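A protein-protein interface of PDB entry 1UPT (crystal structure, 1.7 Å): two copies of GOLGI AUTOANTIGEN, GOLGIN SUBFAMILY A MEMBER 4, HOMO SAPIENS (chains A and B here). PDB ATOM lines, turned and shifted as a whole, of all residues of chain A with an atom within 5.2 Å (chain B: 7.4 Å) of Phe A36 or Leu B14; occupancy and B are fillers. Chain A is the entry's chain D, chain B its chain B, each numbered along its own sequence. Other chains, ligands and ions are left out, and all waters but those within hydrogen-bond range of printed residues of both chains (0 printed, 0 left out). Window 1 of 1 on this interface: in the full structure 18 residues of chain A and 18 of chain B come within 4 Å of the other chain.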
ATOM      1  N   LEU A  14      25.076   1.506  -9.801  1.00  0.00           N
ATOM      2  CA  LEU A  14      26.143   0.695 -10.358  1.00  0.00           C
ATOM      3  C   LEU A  14      26.622   1.147 -11.742  1.00  0.00           C
ATOM      4  O   LEU A  14      27.815   1.063 -11.997  1.00  0.00           O
ATOM      5  CB  LEU A  14      25.774  -0.780 -10.359  1.00  0.00           C
ATOM      6  CG  LEU A  14      26.075  -1.394  -8.999  1.00  0.00           C
ATOM      7  CD1 LEU A  14      25.354  -2.688  -8.827  1.00  0.00           C
ATOM      8  CD2 LEU A  14      27.613  -1.557  -8.847  1.00  0.00           C
ATOM      9  N   ILE A  30      25.995   1.473  -2.378  1.00  0.00           N
ATOM     10  CA  ILE A  30      25.947   0.050  -2.709  1.00  0.00           C
ATOM     11  C   ILE A  30      26.064  -0.780  -1.466  1.00  0.00           C
ATOM     12  O   ILE A  30      25.305  -1.743  -1.266  1.00  0.00           O
ATOM     13  CB  ILE A  30      27.096  -0.311  -3.681  1.00  0.00           C
ATOM     14  CG1 ILE A  30      26.850   0.350  -5.026  1.00  0.00           C
ATOM     15  CG2 ILE A  30      27.190  -1.798  -3.834  1.00  0.00           C
ATOM     16  CD1 ILE A  30      28.072   0.458  -5.903  1.00  0.00           C
ATOM     17  N   THR A  31      27.013  -0.420  -0.611  1.00  0.00           N
ATOM     18  CA  THR A  31      27.236  -1.195   0.607  1.00  0.00           C
ATOM     19  C   THR A  31      26.064  -1.100   1.591  1.00  0.00           C
ATOM     20  O   THR A  31      25.796  -2.043   2.346  1.00  0.00           O
ATOM     21  CB  THR A  31      28.566  -0.796   1.297  1.00  0.00           C
ATOM     22  OG1 THR A  31      28.686   0.623   1.376  1.00  0.00           O
ATOM     23  CG2 THR A  31      29.760  -1.236   0.458  1.00  0.00           C
ATOM     24  N   LEU A  34      22.774  -2.969  -0.238  1.00  0.00           N
ATOM     25  CA  LEU A  34      22.940  -4.431  -0.242  1.00  0.00           C
ATOM     26  C   LEU A  34      23.217  -5.033   1.139  1.00  0.00           C
ATOM     27  O   LEU A  34      23.371  -6.235   1.252  1.00  0.00           O
ATOM     28  CB  LEU A  34      24.019  -4.858  -1.254  1.00  0.00           C
ATOM     29  CG  LEU A  34      23.471  -4.992  -2.681  1.00  0.00           C
ATOM     30  CD1 LEU A  34      24.585  -5.085  -3.683  1.00  0.00           C
ATOM     31  CD2 LEU A  34      22.542  -6.195  -2.786  1.00  0.00           C
ATOM     32  N   LYS A  35      23.261  -4.204   2.184  1.00  0.00           N
ATOM     33  CA  LYS A  35      23.344  -4.694   3.565  1.00  0.00           C
ATOM     34  C   LYS A  35      24.566  -5.596   3.761  1.00  0.00           C
ATOM     35  O   LYS A  35      24.457  -6.704   4.297  1.00  0.00           O
ATOM     36  CB  LYS A  35      22.048  -5.445   3.978  1.00  0.00           C
ATOM     37  CG  LYS A  35      20.737  -4.720   3.628  1.00  0.00           C
ATOM     38  CD  LYS A  35      19.590  -5.044   4.612  1.00  0.00           C
ATOM     39  CE  LYS A  35      18.313  -4.222   4.308  1.00  0.00           C
ATOM     40  NZ  LYS A  35      18.528  -2.730   4.410  1.00  0.00           N
ATOM     41  N   PHE A  36      25.732  -5.120   3.330  1.00  0.00           N
ATOM     42  CA  PHE A  36      26.971  -5.860   3.533  1.00  0.00           C
ATOM     43  C   PHE A  36      27.291  -5.909   5.024  1.00  0.00           C
ATOM     44  O   PHE A  36      27.036  -4.930   5.719  1.00  0.00           O
ATOM     45  CB  PHE A  36      28.141  -5.178   2.832  1.00  0.00           C
ATOM     46  CG  PHE A  36      28.211  -5.439   1.361  1.00  0.00           C
ATOM     47  CD1 PHE A  36      27.364  -4.784   0.491  1.00  0.00           C
ATOM     48  CD2 PHE A  36      29.153  -6.313   0.848  1.00  0.00           C
ATOM     49  CE1 PHE A  36      27.445  -5.008  -0.880  1.00  0.00           C
ATOM     50  CE2 PHE A  36      29.245  -6.544  -0.518  1.00  0.00           C
ATOM     51  CZ  PHE A  36      28.387  -5.892  -1.385  1.00  0.00           C
ATOM     52  N   PRO A  37      27.849  -7.015   5.508  1.00  0.00           N
ATOM     53  CA  PRO A  37      28.357  -7.067   6.886  1.00  0.00           C
ATOM     54  C   PRO A  37      29.381  -5.946   7.114  1.00  0.00           C
ATOM     55  O   PRO A  37      30.153  -5.642   6.196  1.00  0.00           O
ATOM     56  CB  PRO A  37      29.040  -8.439   6.968  1.00  0.00           C
ATOM     57  CG  PRO A  37      28.477  -9.257   5.859  1.00  0.00           C
ATOM     58  CD  PRO A  37      28.048  -8.289   4.792  1.00  0.00           C
ATOM     59  N   ASP A  38      29.390  -5.347   8.305  1.00  0.00           N
ATOM     60  CA  ASP A  38      30.192  -4.135   8.562  1.00  0.00           C
ATOM     61  C   ASP A  38      31.672  -4.315   8.258  1.00  0.00           C
ATOM     62  O   ASP A  38      32.343  -3.379   7.827  1.00  0.00           O
ATOM     63  CB  ASP A  38      30.042  -3.664  10.010  1.00  0.00           C
ATOM     64  CG  ASP A  38      28.599  -3.544  10.433  1.00  0.00           C
ATOM     65  OD1 ASP A  38      28.258  -4.065  11.518  1.00  0.00           O
ATOM     66  OD2 ASP A  38      27.727  -2.977   9.735  1.00  0.00           O
ATOM     67  N   GLN A  40      33.043  -6.285   5.857  1.00  0.00           N
ATOM     68  CA  GLN A  40      33.231  -6.209   4.409  1.00  0.00           C
ATOM     69  C   GLN A  40      33.114  -4.777   3.920  1.00  0.00           C
ATOM     70  O   GLN A  40      33.885  -4.345   3.071  1.00  0.00           O
ATOM     71  CB  GLN A  40      32.250  -7.125   3.690  1.00  0.00           C
ATOM     72  CG  GLN A  40      32.705  -8.566   3.705  1.00  0.00           C
ATOM     73  CD  GLN A  40      31.823  -9.468   2.874  1.00  0.00           C
ATOM     74  OE1 GLN A  40      30.658  -9.183   2.691  1.00  0.00           O
ATOM     75  NE2 GLN A  40      32.381 -10.549   2.373  1.00  0.00           N
ATOM     76  N   THR A  41      32.149  -4.041   4.464  1.00  0.00           N
ATOM     77  CA  THR A  41      31.948  -2.646   4.119  1.00  0.00           C
ATOM     78  C   THR A  41      33.213  -1.840   4.406  1.00  0.00           C
ATOM     79  O   THR A  41      33.653  -1.032   3.580  1.00  0.00           O
ATOM     80  CB  THR A  41      30.757  -2.065   4.915  1.00  0.00           C
ATOM     81  OG1 THR A  41      29.518  -2.655   4.465  1.00  0.00           O
ATOM     82  CG2 THR A  41      30.604  -0.554   4.661  1.00  0.00           C
ATOM     83  N   ILE A  44      35.786  -2.614   1.795  1.00  0.00           N
ATOM     84  CA  ILE A  44      35.439  -2.038   0.503  1.00  0.00           C
ATOM     85  C   ILE A  44      35.705  -0.529   0.508  1.00  0.00           C
ATOM     86  O   ILE A  44      36.278  -0.001  -0.419  1.00  0.00           O
ATOM     87  CB  ILE A  44      33.954  -2.344   0.145  1.00  0.00           C
ATOM     88  CG1 ILE A  44      33.770  -3.808  -0.258  1.00  0.00           C
ATOM     89  CG2 ILE A  44      33.491  -1.459  -0.976  1.00  0.00           C
ATOM     90  CD1 ILE A  44      32.352  -4.313  -0.001  1.00  0.00           C
ATOM     91  N   PHE B   7      20.231 -10.708  -3.713  1.00  0.00           N
ATOM     92  CA  PHE B   7      21.045  -9.886  -2.810  1.00  0.00           C
ATOM     93  C   PHE B   7      22.226 -10.621  -2.260  1.00  0.00           C
ATOM     94  O   PHE B   7      23.321 -10.076  -2.199  1.00  0.00           O
ATOM     95  CB  PHE B   7      20.227  -9.371  -1.630  1.00  0.00           C
ATOM     96  CG  PHE B   7      19.417  -8.149  -1.929  1.00  0.00           C
ATOM     97  CD1 PHE B   7      18.835  -7.953  -3.175  1.00  0.00           C
ATOM     98  CD2 PHE B   7      19.222  -7.191  -0.946  1.00  0.00           C
ATOM     99  CE1 PHE B   7      18.083  -6.843  -3.434  1.00  0.00           C
ATOM    100  CE2 PHE B   7      18.457  -6.058  -1.202  1.00  0.00           C
ATOM    101  CZ  PHE B   7      17.886  -5.890  -2.449  1.00  0.00           C
ATOM    102  N   GLU B   8      21.996 -11.850  -1.808  1.00  0.00           N
ATOM    103  CA  GLU B   8      23.080 -12.710  -1.359  1.00  0.00           C
ATOM    104  C   GLU B   8      24.081 -12.963  -2.490  1.00  0.00           C
ATOM    105  O   GLU B   8      25.290 -12.886  -2.302  1.00  0.00           O
ATOM    106  CB  GLU B   8      22.524 -14.041  -0.877  1.00  0.00           C
ATOM    107  CG  GLU B   8      23.513 -14.859  -0.058  1.00  0.00           C
ATOM    108  CD  GLU B   8      22.851 -16.065   0.626  1.00  0.00           C
ATOM    109  OE1 GLU B   8      21.584 -16.140   0.683  1.00  0.00           O
ATOM    110  OE2 GLU B   8      23.605 -16.936   1.125  1.00  0.00           O
ATOM    111  N   TYR B   9      23.554 -13.235  -3.671  1.00  0.00           N
ATOM    112  CA  TYR B   9      24.393 -13.510  -4.832  1.00  0.00           C
ATOM    113  C   TYR B   9      25.201 -12.266  -5.164  1.00  0.00           C
ATOM    114  O   TYR B   9      26.401 -12.328  -5.307  1.00  0.00           O
ATOM    115  CB  TYR B   9      23.523 -13.934  -6.015  1.00  0.00           C
ATOM    116  CG  TYR B   9      24.320 -14.512  -7.139  1.00  0.00           C
ATOM    117  CD1 TYR B   9      24.498 -15.869  -7.253  1.00  0.00           C
ATOM    118  CD2 TYR B   9      24.936 -13.695  -8.051  1.00  0.00           C
ATOM    119  CE1 TYR B   9      25.238 -16.420  -8.304  1.00  0.00           C
ATOM    120  CE2 TYR B   9      25.696 -14.233  -9.101  1.00  0.00           C
ATOM    121  CZ  TYR B   9      25.852 -15.578  -9.207  1.00  0.00           C
ATOM    122  OH  TYR B   9      26.590 -16.098 -10.224  1.00  0.00           O
ATOM    123  N   LEU B  10      24.530 -11.128  -5.235  1.00  0.00           N
ATOM    124  CA  LEU B  10      25.163  -9.850  -5.570  1.00  0.00           C
ATOM    125  C   LEU B  10      26.221  -9.408  -4.576  1.00  0.00           C
ATOM    126  O   LEU B  10      27.190  -8.772  -4.982  1.00  0.00           O
ATOM    127  CB  LEU B  10      24.122  -8.724  -5.722  1.00  0.00           C
ATOM    128  CG  LEU B  10      23.466  -8.457  -7.082  1.00  0.00           C
ATOM    129  CD1 LEU B  10      22.646  -7.213  -6.984  1.00  0.00           C
ATOM    130  CD2 LEU B  10      24.509  -8.276  -8.175  1.00  0.00           C
ATOM    131  N   ARG B  11      26.060  -9.733  -3.292  1.00  0.00           N
ATOM    132  CA  ARG B  11      27.063  -9.393  -2.277  1.00  0.00           C
ATOM    133  C   ARG B  11      28.366 -10.146  -2.454  1.00  0.00           C
ATOM    134  O   ARG B  11      29.446  -9.576  -2.309  1.00  0.00           O
ATOM    135  CB  ARG B  11      26.530  -9.655  -0.847  1.00  0.00           C
ATOM    136  CG  ARG B  11      25.605  -8.580  -0.305  1.00  0.00           C
ATOM    137  CD  ARG B  11      25.438  -8.635   1.233  1.00  0.00           C
ATOM    138  NE  ARG B  11      24.746  -9.858   1.643  1.00  0.00           N
ATOM    139  CZ  ARG B  11      23.431 -10.008   1.723  1.00  0.00           C
ATOM    140  NH1 ARG B  11      22.610  -9.017   1.415  1.00  0.00           N
ATOM    141  NH2 ARG B  11      22.926 -11.182   2.093  1.00  0.00           N
ATOM    142  N   LYS B  12      28.266 -11.430  -2.760  1.00  0.00           N
ATOM    143  CA  LYS B  12      29.432 -12.258  -3.038  1.00  0.00           C
ATOM    144  C   LYS B  12      30.186 -11.704  -4.256  1.00  0.00           C
ATOM    145  O   LYS B  12      31.398 -11.514  -4.226  1.00  0.00           O
ATOM    146  CB  LYS B  12      28.971 -13.700  -3.291  1.00  0.00           C
ATOM    147  CG  LYS B  12      30.037 -14.622  -3.859  1.00  0.00           C
ATOM    148  CD  LYS B  12      30.772 -15.413  -2.774  1.00  0.00           C
ATOM    149  CE  LYS B  12      32.178 -15.769  -3.237  1.00  0.00           C
ATOM    150  NZ  LYS B  12      32.935 -16.446  -2.172  1.00  0.00           N
ATOM    151  N   VAL B  13      29.431 -11.411  -5.303  1.00  0.00           N
ATOM    152  CA  VAL B  13      29.993 -10.956  -6.568  1.00  0.00           C
ATOM    153  C   VAL B  13      30.539  -9.520  -6.447  1.00  0.00           C
ATOM    154  O   VAL B  13      31.616  -9.200  -6.946  1.00  0.00           O
ATOM    155  CB  VAL B  13      28.905 -11.070  -7.643  1.00  0.00           C
ATOM    156  CG1 VAL B  13      29.264 -10.320  -8.873  1.00  0.00           C
ATOM    157  CG2 VAL B  13      28.634 -12.521  -7.927  1.00  0.00           C
ATOM    158  N   LEU B  14      29.815  -8.663  -5.752  1.00  0.00           N
ATOM    159  CA  LEU B  14      30.224  -7.272  -5.626  1.00  0.00           C
ATOM    160  C   LEU B  14      31.406  -7.157  -4.708  1.00  0.00           C
ATOM    161  O   LEU B  14      32.218  -6.274  -4.880  1.00  0.00           O
ATOM    162  CB  LEU B  14      29.093  -6.376  -5.132  1.00  0.00           C
ATOM    163  CG  LEU B  14      28.284  -5.827  -6.294  1.00  0.00           C
ATOM    164  CD1 LEU B  14      26.971  -5.360  -5.802  1.00  0.00           C
ATOM    165  CD2 LEU B  14      29.041  -4.724  -7.037  1.00  0.00           C
ATOM    166  N   PHE B  15      31.520  -8.058  -3.739  1.00  0.00           N
ATOM    167  CA  PHE B  15      32.638  -7.991  -2.831  1.00  0.00           C
ATOM    168  C   PHE B  15      33.924  -8.268  -3.591  1.00  0.00           C
ATOM    169  O   PHE B  15      34.858  -7.500  -3.489  1.00  0.00           O
ATOM    170  CB  PHE B  15      32.476  -8.932  -1.635  1.00  0.00           C
ATOM    171  CG  PHE B  15      33.642  -8.877  -0.684  1.00  0.00           C
ATOM    172  CD1 PHE B  15      33.917  -7.714   0.025  1.00  0.00           C
ATOM    173  CD2 PHE B  15      34.488  -9.971  -0.532  1.00  0.00           C
ATOM    174  CE1 PHE B  15      35.008  -7.639   0.874  1.00  0.00           C
ATOM    175  CE2 PHE B  15      35.587  -9.907   0.327  1.00  0.00           C
ATOM    176  CZ  PHE B  15      35.845  -8.731   1.033  1.00  0.00           C
ATOM    177  N   GLU B  16      33.946  -9.342  -4.378  1.00  0.00           N
ATOM    178  CA  GLU B  16      35.110  -9.635  -5.231  1.00  0.00           C
ATOM    179  C   GLU B  16      35.422  -8.475  -6.186  1.00  0.00           C
ATOM    180  O   GLU B  16      36.553  -8.035  -6.282  1.00  0.00           O
ATOM    181  CB  GLU B  16      34.926 -10.938  -6.019  1.00  0.00           C
ATOM    182  CG  GLU B  16      34.664 -12.173  -5.166  1.00  0.00           C
ATOM    183  CD  GLU B  16      35.840 -12.478  -4.264  1.00  0.00           C
ATOM    184  OE1 GLU B  16      36.890 -12.865  -4.808  1.00  0.00           O
ATOM    185  OE2 GLU B  16      35.737 -12.271  -3.036  1.00  0.00           O
ATOM    186  N   TYR B  17      34.405  -7.944  -6.847  1.00  0.00           N
ATOM    187  CA  TYR B  17      34.598  -6.841  -7.782  1.00  0.00           C
ATOM    188  C   TYR B  17      35.184  -5.577  -7.134  1.00  0.00           C
ATOM    189  O   TYR B  17      36.139  -4.993  -7.626  1.00  0.00           O
ATOM    190  CB  TYR B  17      33.273  -6.504  -8.460  1.00  0.00           C
ATOM    191  CG  TYR B  17      33.352  -5.367  -9.434  1.00  0.00           C
ATOM    192  CD1 TYR B  17      33.961  -5.509 -10.670  1.00  0.00           C
ATOM    193  CD2 TYR B  17      32.788  -4.140  -9.129  1.00  0.00           C
ATOM    194  CE1 TYR B  17      34.033  -4.441 -11.559  1.00  0.00           C
ATOM    195  CE2 TYR B  17      32.852  -3.084 -10.009  1.00  0.00           C
ATOM    196  CZ  TYR B  17      33.481  -3.233 -11.211  1.00  0.00           C
ATOM    197  OH  TYR B  17      33.498  -2.156 -12.059  1.00  0.00           O
ATOM    198  N   MET B  18      34.601  -5.179  -6.018  1.00  0.00           N
ATOM    199  CA  MET B  18      35.003  -3.971  -5.325  1.00  0.00           C
ATOM    200  C   MET B  18      36.360  -4.124  -4.648  1.00  0.00           C
ATOM    201  O   MET B  18      37.024  -3.143  -4.434  1.00  0.00           O
ATOM    202  CB  MET B  18      33.909  -3.551  -4.332  1.00  0.00           C
ATOM    203  CG  MET B  18      32.688  -3.090  -5.092  1.00  0.00           C
ATOM    204  SD  MET B  18      31.165  -2.703  -3.968  1.00  0.00           S
ATOM    205  CE  MET B  18      31.222  -0.768  -4.042  1.00  0.00           C
ATOM    206  N   MET B  19      36.783  -5.365  -4.396  1.00  0.00           N
ATOM    207  CA  MET B  19      38.117  -5.685  -3.853  1.00  0.00           C
ATOM    208  C   MET B  19      39.173  -5.934  -4.946  1.00  0.00           C
ATOM    209  O   MET B  19      40.318  -6.247  -4.643  1.00  0.00           O
ATOM    210  CB  MET B  19      38.015  -6.890  -2.920  1.00  0.00           C
ATOM    211  CG  MET B  19      37.203  -6.616  -1.646  1.00  0.00           C
ATOM    212  SD  MET B  19      37.867  -5.013  -0.708  1.00  0.00           S
ATOM    213  CE  MET B  19      39.532  -5.867   0.086  1.00  0.00           C
ATOM    214  N   GLY B  20      38.768  -5.782  -6.210  1.00  0.00           N
ATOM    215  CA  GLY B  20      39.652  -5.798  -7.357  1.00  0.00           C
ATOM    216  C   GLY B  20      40.013  -7.182  -7.857  1.00  0.00           C
ATOM    217  O   GLY B  20      41.017  -7.346  -8.564  1.00  0.00           O
ATOM    218  N   MET B  26      33.385 -10.571 -12.913  1.00  0.00           N
ATOM    219  CA  MET B  26      32.419  -9.979 -11.985  1.00  0.00           C
ATOM    220  C   MET B  26      31.588  -8.886 -12.665  1.00  0.00           C
ATOM    221  O   MET B  26      30.397  -8.771 -12.394  1.00  0.00           O
ATOM    222  CB  MET B  26      33.094  -9.425 -10.731  1.00  0.00           C
ATOM    223  CG  MET B  26      33.835 -10.417  -9.798  1.00  0.00           C
ATOM    224  SD  MET B  26      32.813 -12.017  -9.239  1.00  0.00           S
ATOM    225  CE  MET B  26      33.143 -13.282 -10.698  1.00  0.00           C
ATOM    226  N   VAL B  29      28.972 -10.585 -14.607  1.00  0.00           N
ATOM    227  CA  VAL B  29      27.948 -11.133 -13.743  1.00  0.00           C
ATOM    228  C   VAL B  29      26.988 -10.025 -13.220  1.00  0.00           C
ATOM    229  O   VAL B  29      25.784 -10.191 -13.245  1.00  0.00           O
ATOM    230  CB  VAL B  29      28.540 -11.842 -12.520  1.00  0.00           C
ATOM    231  CG1 VAL B  29      27.431 -12.294 -11.602  1.00  0.00           C
ATOM    232  CG2 VAL B  29      29.401 -13.041 -12.919  1.00  0.00           C
ATOM    233  N   ILE B  30      27.542  -8.917 -12.749  1.00  0.00           N
ATOM    234  CA  ILE B  30      26.754  -7.859 -12.138  1.00  0.00           C
ATOM    235  C   ILE B  30      25.804  -7.278 -13.172  1.00  0.00           C
ATOM    236  O   ILE B  30      24.634  -7.091 -12.881  1.00  0.00           O
ATOM    237  CB  ILE B  30      27.642  -6.735 -11.565  1.00  0.00           C
ATOM    238  CG1 ILE B  30      28.456  -7.228 -10.360  1.00  0.00           C
ATOM    239  CG2 ILE B  30      26.800  -5.530 -11.195  1.00  0.00           C
ATOM    240  CD1 ILE B  30      29.703  -6.378 -10.062  1.00  0.00           C
ATOM    241  N   LEU B  34      21.569  -7.727 -12.767  1.00  0.00           N
ATOM    242  CA  LEU B  34      20.765  -6.512 -12.661  1.00  0.00           C
ATOM    243  C   LEU B  34      20.123  -6.087 -13.977  1.00  0.00           C
ATOM    244  O   LEU B  34      19.557  -5.019 -14.061  1.00  0.00           O
ATOM    245  CB  LEU B  34      21.617  -5.375 -12.080  1.00  0.00           C
ATOM    246  CG  LEU B  34      21.921  -5.502 -10.579  1.00  0.00           C
ATOM    247  CD1 LEU B  34      23.037  -4.565 -10.205  1.00  0.00           C
ATOM    248  CD2 LEU B  34      20.676  -5.234  -9.718  1.00  0.00           C
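O of Leu A34 is in hydrogen-bond range of NH1 of Arg B11.
O of Thr A31 lies within hydrogen-bond range of N of Phe A36 (3.2 Å).
Among the printed residues, pairs that only touch across the chains: Leu A34 with Leu B14 (3.2 Å), Leu A14 with Leu B34 (3.3 Å), Phe A36 with Arg B11 (3.5 Å), Gln A40 with Phe B15 (3.6 Å), Ile A44 with Phe B15 (3.7 Å), Lys A35 with Arg B11 (3.8 Å), Leu A34 with Phe B7 (3.8 Å), Phe A36 with Leu B14 (3.8 Å), Ile A30 with Met B18 (3.9 Å), Ile A44 with Met B18 (3.9 Å), Leu A14 with Leu B14 (3.9 Å) and Leu A14 with Ile B30 (3.97 Å).
Of chain B, only Arg B11 and Leu B14 come within 4 Å of Phe A36. Leu B14 touches three residues of chain A. Printed residues of chain A within 4 Å of Ile B30: Leu A14. Printed residues of chain B within 4 Å of Gln A40: Phe B15 (3.6 Å). Of the printed residues of chain A, Arg B11 touches Leu A34 (2.9 Å), Lys A35 (3.8 Å) and Phe A36 (3.5 Å). Printed residues of chain A within 4 Å of Leu B34: Leu A14. Printed residues of chain A within 4 Å of Met B18: Ile A30 and Ile A44. Pro A37 touches none of the printed residues of chain B. The nearest residue of chain B that does not touch Phe A36 is Phe B15 (4.2 Å).
Hydrophobic or aromatic side chains of chain A that line the printed part of chain B: Leu A14, Ile A30, Leu A34, Phe A36 and Ile A44. Of the 18 printed residues of chain B, 7 touch a printed residue of chain A. Hydrophobic or aromatic side chains of chain B within 4 Å of the printed part of chain A: Phe B7, Leu B14, Phe B15, Met B18, Ile B30 and Leu B34.
Leu B14 touches its own counterpart, Leu A14. Leu A14 touches Ile B30, but with the chains exchanged Ile A30 does not touch Leu B14 (4.1 Å). Leu A14 touches Leu B34, and with the chains exchanged Leu A34 touches Leu B14. Of the 13 pairs that touch across the chains among the printed residues, 3 have their exchanged pair printed and touching as well.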
